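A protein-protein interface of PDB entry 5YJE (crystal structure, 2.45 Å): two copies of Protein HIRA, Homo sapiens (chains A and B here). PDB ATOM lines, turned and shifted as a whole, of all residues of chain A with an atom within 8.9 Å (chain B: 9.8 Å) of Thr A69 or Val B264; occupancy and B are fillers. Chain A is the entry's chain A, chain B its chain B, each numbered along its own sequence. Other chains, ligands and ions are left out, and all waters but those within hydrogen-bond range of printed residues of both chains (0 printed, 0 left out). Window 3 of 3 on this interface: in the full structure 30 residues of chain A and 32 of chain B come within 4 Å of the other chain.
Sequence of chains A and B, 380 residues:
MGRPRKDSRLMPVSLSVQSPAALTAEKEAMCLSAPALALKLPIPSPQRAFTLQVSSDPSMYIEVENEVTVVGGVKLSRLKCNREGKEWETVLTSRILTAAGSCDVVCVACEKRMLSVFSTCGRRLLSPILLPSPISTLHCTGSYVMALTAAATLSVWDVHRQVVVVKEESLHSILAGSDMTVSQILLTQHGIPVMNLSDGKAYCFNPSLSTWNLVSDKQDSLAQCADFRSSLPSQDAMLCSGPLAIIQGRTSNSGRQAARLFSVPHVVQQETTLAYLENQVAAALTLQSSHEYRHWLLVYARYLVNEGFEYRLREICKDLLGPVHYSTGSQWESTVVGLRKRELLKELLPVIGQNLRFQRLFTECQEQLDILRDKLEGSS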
ATOM      1  N   GLU A  65       8.866   3.682 -10.917  1.00  0.00           N
ATOM      2  CA  GLU A  65       9.477   4.506  -9.885  1.00  0.00           C
ATOM      3  C   GLU A  65      10.153   5.681 -10.560  1.00  0.00           C
ATOM      4  O   GLU A  65      11.087   5.497 -11.342  1.00  0.00           O
ATOM      5  CB  GLU A  65      10.489   3.721  -9.047  1.00  0.00           C
ATOM      6  CG  GLU A  65      10.050   2.385  -8.509  1.00  0.00           C
ATOM      7  CD  GLU A  65      11.255   1.585  -8.011  1.00  0.00           C
ATOM      8  OE1 GLU A  65      12.296   2.207  -7.672  1.00  0.00           O
ATOM      9  OE2 GLU A  65      11.172   0.338  -7.970  1.00  0.00           O
ATOM     10  N   ASN A  66       9.717   6.886 -10.234  1.00  0.00           N
ATOM     11  CA  ASN A  66      10.132   8.052 -10.987  1.00  0.00           C
ATOM     12  C   ASN A  66      11.345   8.722 -10.356  1.00  0.00           C
ATOM     13  O   ASN A  66      11.343   9.032  -9.162  1.00  0.00           O
ATOM     14  CB  ASN A  66       8.967   9.032 -11.117  1.00  0.00           C
ATOM     15  CG  ASN A  66       8.038   8.660 -12.263  1.00  0.00           C
ATOM     16  OD1 ASN A  66       8.504   8.303 -13.347  1.00  0.00           O
ATOM     17  ND2 ASN A  66       6.730   8.718 -12.027  1.00  0.00           N
ATOM     18  N   GLU A  67      12.374   8.943 -11.172  1.00  0.00           N
ATOM     19  CA  GLU A  67      13.549   9.707 -10.770  1.00  0.00           C
ATOM     20  C   GLU A  67      14.288   9.049  -9.600  1.00  0.00           C
ATOM     21  O   GLU A  67      14.664   9.700  -8.626  1.00  0.00           O
ATOM     22  CB  GLU A  67      13.159  11.147 -10.453  1.00  0.00           C
ATOM     23  CG  GLU A  67      12.629  11.878 -11.655  1.00  0.00           C
ATOM     24  CD  GLU A  67      12.219  13.298 -11.336  1.00  0.00           C
ATOM     25  OE1 GLU A  67      12.729  14.229 -12.000  1.00  0.00           O
ATOM     26  OE2 GLU A  67      11.384  13.479 -10.420  1.00  0.00           O
ATOM     27  N   VAL A  68      14.527   7.741  -9.724  1.00  0.00           N
ATOM     28  CA  VAL A  68      15.170   6.983  -8.660  1.00  0.00           C
ATOM     29  C   VAL A  68      16.682   7.117  -8.619  1.00  0.00           C
ATOM     30  O   VAL A  68      17.286   6.713  -7.617  1.00  0.00           O
ATOM     31  CB  VAL A  68      14.886   5.481  -8.782  1.00  0.00           C
ATOM     32  CG1 VAL A  68      13.428   5.275  -8.979  1.00  0.00           C
ATOM     33  CG2 VAL A  68      15.678   4.903  -9.946  1.00  0.00           C
ATOM     34  N   THR A  69      17.312   7.639  -9.672  1.00  0.00           N
ATOM     35  CA  THR A  69      18.769   7.656  -9.746  1.00  0.00           C
ATOM     36  C   THR A  69      19.180   8.618 -10.852  1.00  0.00           C
ATOM     37  O   THR A  69      18.354   9.060 -11.650  1.00  0.00           O
ATOM     38  CB  THR A  69      19.340   6.252  -9.991  1.00  0.00           C
ATOM     39  OG1 THR A  69      20.767   6.318 -10.001  1.00  0.00           O
ATOM     40  CG2 THR A  69      18.874   5.705 -11.326  1.00  0.00           C
ATOM     41  N   VAL A  70      20.469   8.942 -10.884  1.00  0.00           N
ATOM     42  CA  VAL A  70      21.026   9.935 -11.794  1.00  0.00           C
ATOM     43  C   VAL A  70      22.279   9.365 -12.441  1.00  0.00           C
ATOM     44  O   VAL A  70      23.144   8.809 -11.756  1.00  0.00           O
ATOM     45  CB  VAL A  70      21.356  11.253 -11.075  1.00  0.00           C
ATOM     46  CG1 VAL A  70      21.660  12.327 -12.095  1.00  0.00           C
ATOM     47  CG2 VAL A  70      20.206  11.665 -10.173  1.00  0.00           C
ATOM     48  N   VAL A  71      22.387   9.525 -13.754  1.00  0.00           N
ATOM     49  CA  VAL A  71      23.441   8.899 -14.541  1.00  0.00           C
ATOM     50  C   VAL A  71      23.854   9.874 -15.632  1.00  0.00           C
ATOM     51  O   VAL A  71      23.038  10.220 -16.491  1.00  0.00           O
ATOM     52  CB  VAL A  71      22.965   7.576 -15.164  1.00  0.00           C
ATOM     53  CG1 VAL A  71      23.850   7.210 -16.322  1.00  0.00           C
ATOM     54  CG2 VAL A  71      22.934   6.460 -14.130  1.00  0.00           C
ATOM     55  N   GLY A  72      25.119  10.296 -15.620  1.00  0.00           N
ATOM     56  CA  GLY A  72      25.625  11.265 -16.580  1.00  0.00           C
ATOM     57  C   GLY A  72      24.832  12.560 -16.616  1.00  0.00           C
ATOM     58  O   GLY A  72      24.750  13.214 -17.662  1.00  0.00           O
ATOM     59  N   GLY A  73      24.226  12.931 -15.485  1.00  0.00           N
ATOM     60  CA  GLY A  73      23.364  14.094 -15.408  1.00  0.00           C
ATOM     61  C   GLY A  73      21.907  13.854 -15.771  1.00  0.00           C
ATOM     62  O   GLY A  73      21.089  14.770 -15.627  1.00  0.00           O
ATOM     63  N   VAL A  74      21.560  12.653 -16.219  1.00  0.00           N
ATOM     64  CA  VAL A  74      20.216  12.302 -16.664  1.00  0.00           C
ATOM     65  C   VAL A  74      19.499  11.568 -15.533  1.00  0.00           C
ATOM     66  O   VAL A  74      19.944  10.495 -15.094  1.00  0.00           O
ATOM     67  CB  VAL A  74      20.280  11.438 -17.936  1.00  0.00           C
ATOM     68  CG1 VAL A  74      18.898  11.170 -18.484  1.00  0.00           C
ATOM     69  CG2 VAL A  74      21.162  12.104 -18.978  1.00  0.00           C
ATOM     70  N   LYS A  75      18.390  12.146 -15.060  1.00  0.00           N
ATOM     71  CA  LYS A  75      17.542  11.485 -14.071  1.00  0.00           C
ATOM     72  C   LYS A  75      16.801  10.319 -14.712  1.00  0.00           C
ATOM     73  O   LYS A  75      16.202  10.465 -15.782  1.00  0.00           O
ATOM     74  CB  LYS A  75      16.538  12.472 -13.481  1.00  0.00           C
ATOM     75  CG  LYS A  75      17.168  13.732 -12.907  1.00  0.00           C
ATOM     76  CD  LYS A  75      16.122  14.775 -12.519  1.00  0.00           C
ATOM     77  CE  LYS A  75      16.800  16.096 -12.148  1.00  0.00           C
ATOM     78  NZ  LYS A  75      15.841  17.213 -11.896  1.00  0.00           N
ATOM     79  N   LEU A  76      16.832   9.160 -14.066  1.00  0.00           N
ATOM     80  CA  LEU A  76      16.253   7.951 -14.628  1.00  0.00           C
ATOM     81  C   LEU A  76      14.964   7.597 -13.912  1.00  0.00           C
ATOM     82  O   LEU A  76      14.827   7.774 -12.702  1.00  0.00           O
ATOM     83  CB  LEU A  76      17.207   6.750 -14.535  1.00  0.00           C
ATOM     84  CG  LEU A  76      18.557   6.798 -15.255  1.00  0.00           C
ATOM     85  CD1 LEU A  76      19.377   5.562 -14.887  1.00  0.00           C
ATOM     86  CD2 LEU A  76      18.404   6.925 -16.772  1.00  0.00           C
ATOM     87  N   SER A  77      14.021   7.072 -14.672  1.00  0.00           N
ATOM     88  CA  SER A  77      12.800   6.530 -14.112  1.00  0.00           C
ATOM     89  C   SER A  77      12.743   5.064 -14.495  1.00  0.00           C
ATOM     90  O   SER A  77      13.236   4.679 -15.554  1.00  0.00           O
ATOM     91  CB  SER A  77      11.589   7.301 -14.604  1.00  0.00           C
ATOM     92  OG  SER A  77      11.658   8.647 -14.152  1.00  0.00           O
ATOM     93  N   ARG A  78      12.215   4.233 -13.604  1.00  0.00           N
ATOM     94  CA  ARG A  78      12.200   2.799 -13.827  1.00  0.00           C
ATOM     95  C   ARG A  78      10.812   2.317 -14.212  1.00  0.00           C
ATOM     96  O   ARG A  78       9.799   2.733 -13.635  1.00  0.00           O
ATOM     97  CB  ARG A  78      12.691   2.027 -12.594  1.00  0.00           C
ATOM     98  CG  ARG A  78      13.982   2.522 -12.024  1.00  0.00           C
ATOM     99  CD  ARG A  78      14.438   1.656 -10.846  1.00  0.00           C
ATOM    100  NE  ARG A  78      14.625   0.259 -11.241  1.00  0.00           N
ATOM    101  CZ  ARG A  78      14.931  -0.725 -10.404  1.00  0.00           C
ATOM    102  NH1 ARG A  78      15.066  -0.468  -9.110  1.00  0.00           N
ATOM    103  NH2 ARG A  78      15.101  -1.946 -10.875  1.00  0.00           N
ATOM    104  N   VAL A  91      14.770   1.578 -18.116  1.00  0.00           N
ATOM    105  CA  VAL A  91      14.851   2.948 -17.637  1.00  0.00           C
ATOM    106  C   VAL A  91      14.375   3.884 -18.752  1.00  0.00           C
ATOM    107  O   VAL A  91      14.508   3.583 -19.940  1.00  0.00           O
ATOM    108  CB  VAL A  91      16.290   3.281 -17.167  1.00  0.00           C
ATOM    109  CG1 VAL A  91      16.667   2.451 -15.908  1.00  0.00           C
ATOM    110  CG2 VAL A  91      17.300   3.027 -18.282  1.00  0.00           C
ATOM    111  N   LEU A  92      13.774   5.004 -18.348  1.00  0.00           N
ATOM    112  CA  LEU A  92      13.414   6.112 -19.222  1.00  0.00           C
ATOM    113  C   LEU A  92      14.044   7.390 -18.674  1.00  0.00           C
ATOM    114  O   LEU A  92      14.385   7.472 -17.493  1.00  0.00           O
ATOM    115  CB  LEU A  92      11.881   6.251 -19.344  1.00  0.00           C
ATOM    116  CG  LEU A  92      11.328   5.083 -20.180  1.00  0.00           C
ATOM    117  CD1 LEU A  92      10.888   3.870 -19.321  1.00  0.00           C
ATOM    118  CD2 LEU A  92      10.258   5.512 -21.200  1.00  0.00           C
ATOM    119  N   THR A  93      14.208   8.398 -19.536  1.00  0.00           N
ATOM    120  CA  THR A  93      14.884   9.619 -19.113  1.00  0.00           C
ATOM    121  C   THR A  93      13.914  10.724 -18.725  1.00  0.00           C
ATOM    122  O   THR A  93      14.313  11.887 -18.629  1.00  0.00           O
ATOM    123  CB  THR A  93      15.862  10.111 -20.185  1.00  0.00           C
ATOM    124  OG1 THR A  93      15.149  10.482 -21.366  1.00  0.00           O
ATOM    125  CG2 THR A  93      16.868   9.025 -20.517  1.00  0.00           C
ATOM    126  N   LEU B 222      21.813   9.155 -23.074  1.00  0.00           N
ATOM    127  CA  LEU B 222      22.460   8.102 -22.313  1.00  0.00           C
ATOM    128  C   LEU B 222      23.749   7.629 -22.961  1.00  0.00           C
ATOM    129  O   LEU B 222      24.368   6.683 -22.462  1.00  0.00           O
ATOM    130  CB  LEU B 222      21.503   6.928 -22.136  1.00  0.00           C
ATOM    131  CG  LEU B 222      20.262   7.246 -21.316  1.00  0.00           C
ATOM    132  CD1 LEU B 222      19.118   6.358 -21.753  1.00  0.00           C
ATOM    133  CD2 LEU B 222      20.558   7.060 -19.834  1.00  0.00           C
ATOM    134  N   CYS B 225      27.256   7.414 -20.940  1.00  0.00           N
ATOM    135  CA  CYS B 225      27.382   6.386 -19.923  1.00  0.00           C
ATOM    136  C   CYS B 225      27.127   4.983 -20.458  1.00  0.00           C
ATOM    137  O   CYS B 225      27.272   4.016 -19.707  1.00  0.00           O
ATOM    138  CB  CYS B 225      26.450   6.707 -18.755  1.00  0.00           C
ATOM    139  SG  CYS B 225      26.946   8.229 -17.889  1.00  0.00           S
ATOM    140  N   ALA B 259      33.402   5.340 -19.528  1.00  0.00           N
ATOM    141  CA  ALA B 259      33.904   5.044 -18.195  1.00  0.00           C
ATOM    142  C   ALA B 259      32.951   4.116 -17.433  1.00  0.00           C
ATOM    143  O   ALA B 259      31.751   4.024 -17.711  1.00  0.00           O
ATOM    144  CB  ALA B 259      34.113   6.342 -17.407  1.00  0.00           C
ATOM    145  N   ARG B 260      33.506   3.416 -16.454  1.00  0.00           N
ATOM    146  CA  ARG B 260      32.674   2.708 -15.497  1.00  0.00           C
ATOM    147  C   ARG B 260      32.084   3.708 -14.511  1.00  0.00           C
ATOM    148  O   ARG B 260      32.735   4.691 -14.140  1.00  0.00           O
ATOM    149  CB  ARG B 260      33.491   1.641 -14.777  1.00  0.00           C
ATOM    150  CG  ARG B 260      33.506   0.298 -15.508  1.00  0.00           C
ATOM    151  CD  ARG B 260      32.115  -0.350 -15.521  1.00  0.00           C
ATOM    152  NE  ARG B 260      32.177  -1.770 -15.181  1.00  0.00           N
ATOM    153  N   LEU B 261      30.835   3.479 -14.122  1.00  0.00           N
ATOM    154  CA  LEU B 261      30.165   4.390 -13.205  1.00  0.00           C
ATOM    155  C   LEU B 261      30.572   4.074 -11.770  1.00  0.00           C
ATOM    156  O   LEU B 261      30.533   2.918 -11.344  1.00  0.00           O
ATOM    157  CB  LEU B 261      28.643   4.314 -13.383  1.00  0.00           C
ATOM    158  CG  LEU B 261      28.184   4.804 -14.774  1.00  0.00           C
ATOM    159  CD1 LEU B 261      26.695   4.628 -15.015  1.00  0.00           C
ATOM    160  CD2 LEU B 261      28.588   6.255 -15.017  1.00  0.00           C
ATOM    161  N   PHE B 262      31.007   5.102 -11.045  1.00  0.00           N
ATOM    162  CA  PHE B 262      31.347   4.981  -9.631  1.00  0.00           C
ATOM    163  C   PHE B 262      30.147   5.176  -8.718  1.00  0.00           C
ATOM    164  O   PHE B 262      30.129   4.647  -7.602  1.00  0.00           O
ATOM    165  CB  PHE B 262      32.425   6.013  -9.259  1.00  0.00           C
ATOM    166  CG  PHE B 262      33.832   5.515  -9.443  1.00  0.00           C
ATOM    167  CD1 PHE B 262      34.150   4.646 -10.477  1.00  0.00           C
ATOM    168  CD2 PHE B 262      34.822   5.880  -8.560  1.00  0.00           C
ATOM    169  CE1 PHE B 262      35.437   4.164 -10.638  1.00  0.00           C
ATOM    170  CE2 PHE B 262      36.109   5.396  -8.717  1.00  0.00           C
ATOM    171  CZ  PHE B 262      36.413   4.531  -9.757  1.00  0.00           C
ATOM    172  N   SER B 263      29.150   5.923  -9.172  1.00  0.00           N
ATOM    173  CA  SER B 263      28.035   6.371  -8.351  1.00  0.00           C
ATOM    174  C   SER B 263      26.861   5.396  -8.319  1.00  0.00           C
ATOM    175  O   SER B 263      25.972   5.560  -7.471  1.00  0.00           O
ATOM    176  CB  SER B 263      27.538   7.715  -8.878  1.00  0.00           C
ATOM    177  OG  SER B 263      27.373   7.619 -10.299  1.00  0.00           O
ATOM    178  N   VAL B 264      26.817   4.416  -9.223  1.00  0.00           N
ATOM    179  CA  VAL B 264      25.693   3.478  -9.299  1.00  0.00           C
ATOM    180  C   VAL B 264      26.213   2.076  -9.517  1.00  0.00           C
ATOM    181  O   VAL B 264      27.283   1.863 -10.115  1.00  0.00           O
ATOM    182  CB  VAL B 264      24.691   3.841 -10.437  1.00  0.00           C
ATOM    183  CG1 VAL B 264      24.081   5.208 -10.212  1.00  0.00           C
ATOM    184  CG2 VAL B 264      25.349   3.756 -11.829  1.00  0.00           C
ATOM    185  N   PRO B 265      25.463   1.074  -9.058  1.00  0.00           N
ATOM    186  CA  PRO B 265      25.844  -0.318  -9.307  1.00  0.00           C
ATOM    187  C   PRO B 265      25.775  -0.674 -10.782  1.00  0.00           C
ATOM    188  O   PRO B 265      25.043  -0.076 -11.571  1.00  0.00           O
ATOM    189  CB  PRO B 265      24.832  -1.142  -8.491  1.00  0.00           C
ATOM    190  CG  PRO B 265      23.773  -0.176  -8.044  1.00  0.00           C
ATOM    191  CD  PRO B 265      24.380   1.193  -8.064  1.00  0.00           C
ATOM    192  N   HIS B 266      26.559  -1.694 -11.133  1.00  0.00           N
ATOM    193  CA  HIS B 266      26.738  -2.093 -12.523  1.00  0.00           C
ATOM    194  C   HIS B 266      25.421  -2.305 -13.267  1.00  0.00           C
ATOM    195  O   HIS B 266      25.338  -2.035 -14.481  1.00  0.00           O
ATOM    196  CB  HIS B 266      27.562  -3.366 -12.572  1.00  0.00           C
ATOM    197  CG  HIS B 266      27.877  -3.820 -13.957  1.00  0.00           C
ATOM    198  ND1 HIS B 266      28.416  -2.977 -14.903  1.00  0.00           N
ATOM    199  CD2 HIS B 266      27.770  -5.034 -14.546  1.00  0.00           C
ATOM    200  CE1 HIS B 266      28.607  -3.647 -16.025  1.00  0.00           C
ATOM    201  NE2 HIS B 266      28.229  -4.899 -15.834  1.00  0.00           N
ATOM    202  N   VAL B 267      24.392  -2.804 -12.571  1.00  0.00           N
ATOM    203  CA  VAL B 267      23.134  -3.102 -13.243  1.00  0.00           C
ATOM    204  C   VAL B 267      22.536  -1.834 -13.858  1.00  0.00           C
ATOM    205  O   VAL B 267      21.938  -1.883 -14.934  1.00  0.00           O
ATOM    206  CB  VAL B 267      22.151  -3.786 -12.269  1.00  0.00           C
ATOM    207  CG1 VAL B 267      21.761  -2.829 -11.151  1.00  0.00           C
ATOM    208  CG2 VAL B 267      20.904  -4.327 -13.041  1.00  0.00           C
ATOM    209  N   VAL B 268      22.697  -0.687 -13.189  1.00  0.00           N
ATOM    210  CA  VAL B 268      22.163   0.565 -13.693  1.00  0.00           C
ATOM    211  C   VAL B 268      22.867   0.954 -14.991  1.00  0.00           C
ATOM    212  O   VAL B 268      22.235   1.453 -15.928  1.00  0.00           O
ATOM    213  CB  VAL B 268      22.289   1.658 -12.617  1.00  0.00           C
ATOM    214  CG1 VAL B 268      21.775   2.978 -13.119  1.00  0.00           C
ATOM    215  CG2 VAL B 268      21.544   1.252 -11.332  1.00  0.00           C
ATOM    216  N   GLN B 269      24.176   0.711 -15.080  1.00  0.00           N
ATOM    217  CA  GLN B 269      24.880   1.023 -16.318  1.00  0.00           C
ATOM    218  C   GLN B 269      24.485   0.054 -17.420  1.00  0.00           C
ATOM    219  O   GLN B 269      24.423   0.440 -18.595  1.00  0.00           O
ATOM    220  CB  GLN B 269      26.402   1.019 -16.112  1.00  0.00           C
ATOM    221  CG  GLN B 269      27.236   1.518 -17.313  1.00  0.00           C
ATOM    222  CD  GLN B 269      28.616   2.038 -16.914  1.00  0.00           C
ATOM    223  OE1 GLN B 269      29.187   1.628 -15.903  1.00  0.00           O
ATOM    224  NE2 GLN B 269      29.161   2.933 -17.716  1.00  0.00           N
ATOM    225  N   GLN B 270      24.211  -1.205 -17.074  1.00  0.00           N
ATOM    226  CA  GLN B 270      23.655  -2.097 -18.084  1.00  0.00           C
ATOM    227  C   GLN B 270      22.297  -1.601 -18.574  1.00  0.00           C
ATOM    228  O   GLN B 270      21.996  -1.682 -19.766  1.00  0.00           O
ATOM    229  CB  GLN B 270      23.528  -3.513 -17.553  1.00  0.00           C
ATOM    230  CG  GLN B 270      24.862  -4.209 -17.271  1.00  0.00           C
ATOM    231  CD  GLN B 270      24.625  -5.610 -16.728  1.00  0.00           C
ATOM    232  OE1 GLN B 270      23.935  -5.778 -15.727  1.00  0.00           O
ATOM    233  NE2 GLN B 270      25.156  -6.620 -17.410  1.00  0.00           N
ATOM    234  N   GLU B 271      21.456  -1.103 -17.674  1.00  0.00           N
ATOM    235  CA  GLU B 271      20.115  -0.738 -18.112  1.00  0.00           C
ATOM    236  C   GLU B 271      20.164   0.530 -18.948  1.00  0.00           C
ATOM    237  O   GLU B 271      19.438   0.651 -19.941  1.00  0.00           O
ATOM    238  CB  GLU B 271      19.168  -0.600 -16.914  1.00  0.00           C
ATOM    239  CG  GLU B 271      19.033  -1.921 -16.124  1.00  0.00           C
ATOM    240  CD  GLU B 271      17.668  -2.154 -15.473  1.00  0.00           C
ATOM    241  OE1 GLU B 271      16.808  -1.236 -15.418  1.00  0.00           O
ATOM    242  OE2 GLU B 271      17.454  -3.295 -15.010  1.00  0.00           O
ATOM    243  N   THR B 272      21.048   1.467 -18.595  1.00  0.00           N
ATOM    244  CA  THR B 272      21.216   2.640 -19.441  1.00  0.00           C
ATOM    245  C   THR B 272      21.816   2.262 -20.784  1.00  0.00           C
ATOM    246  O   THR B 272      21.403   2.795 -21.817  1.00  0.00           O
ATOM    247  CB  THR B 272      22.062   3.704 -18.751  1.00  0.00           C
ATOM    248  OG1 THR B 272      23.382   3.200 -18.554  1.00  0.00           O
ATOM    249  CG2 THR B 272      21.455   4.104 -17.419  1.00  0.00           C
ATOM    250  N   THR B 273      22.750   1.312 -20.797  1.00  0.00           N
ATOM    251  CA  THR B 273      23.346   0.881 -22.057  1.00  0.00           C
ATOM    252  C   THR B 273      22.302   0.224 -22.957  1.00  0.00           C
ATOM    253  O   THR B 273      22.242   0.507 -24.162  1.00  0.00           O
ATOM    254  CB  THR B 273      24.521  -0.066 -21.786  1.00  0.00           C
ATOM    255  OG1 THR B 273      25.540   0.650 -21.089  1.00  0.00           O
ATOM    256  CG2 THR B 273      25.120  -0.605 -23.078  1.00  0.00           C
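CG1 of Val B264 touches OG1 of Thr A69 (3.5 Å). CG1 of Val A71 touches CB of Cys B225, at 3.6 Å. CG2 of Val A71 touches CG1 of Val B268 (3.8 Å). Leu A76 touches Leu B222 (CD2 to CD2, 3.7 Å). CD1 of Leu A76 touches CG1 of Val B268 (3.9 Å). Leu A76 touches Thr B272 (CD1 to CG2, 3.6 Å). CG2 of Val A91 touches O of Glu B271 (3.6 Å). Thr A93 touches Leu B222 (CG2 to CD1, 3.7 Å).
Along chain A the printed residues that touch a printed residue of chain B span positions 69 to 93. Printed residues of chain B that touch a printed residue of chain A: Leu B222, Cys B225, Val B264, Val B268, Glu B271 and Thr B272. Hydrophobic or aromatic side chains of chain B within 4 Å of the printed part of chain A: Leu B222, Val B264 and Val B268. Among the printed residues, 9 pairs touch across the chains. Among the printed residues, no Asp or Glu carboxylate lies within 4 Å of a Lys or Arg side-chain nitrogen of the other chain.
Of chain B, only Val B264 comes within 4 Å of Thr A69. Val B264 touches just one residue of chain A: Thr A69. No residue of chain B comes within 4 Å of Val A70. Leu A76 touches just these residues of chain B: Leu B222, Val B268 and Thr B272. No residue of chain A comes within 4 Å of Ser B263. No residue of chain A comes within 4 Å of Pro B265. Printed residues of chain A within 4 Å of Thr B272: Leu A76. Printed residues of chain B within 4 Å of Val A71: Cys B225 and Val B268. Printed residues of chain B within 4 Å of Gly A72: Cys B225. Of the printed residues of chain B, Val A91 touches Glu B271 (3.6 Å). Printed residues of chain B within 4 Å of Thr A93: Leu B222 (3.7 Å). Gly A73 touches none of the printed residues of chain B. Gln B270 touches none of the printed residues of chain A. The nearest printed residue of chain A that does not touch Thr B272 is Val A91 (4.1 Å).
The backbone NH (N) of Gly A72 sits close to the side-chain sulfur (SG) of Cys B225, 3.6 Å away.
No position is printed for both chains. Of the 9 pairs that touch across the chains among the printed residues, none has its exchanged pair printed and touching as well.
NE2 of Gln B269 lies within hydrogen-bond range of O of Cys B225, at 3.0 Å. The side-chain hydroxyl (OG1) of Thr B272 lies within hydrogen-bond range of the backbone carbonyl oxygen (O) of Gln B269 (3.0 Å). O of Thr A69 is in hydrogen-bond range of N of Leu A76. The backbone NH of Glu A67 sits close to the backbone carbonyl oxygen of Leu A76. OG1 of Thr B272 sits close to O of Val B268 (3.4 Å). N of Val A68 is in hydrogen-bond range of O of Leu A76 (3.0 Å).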
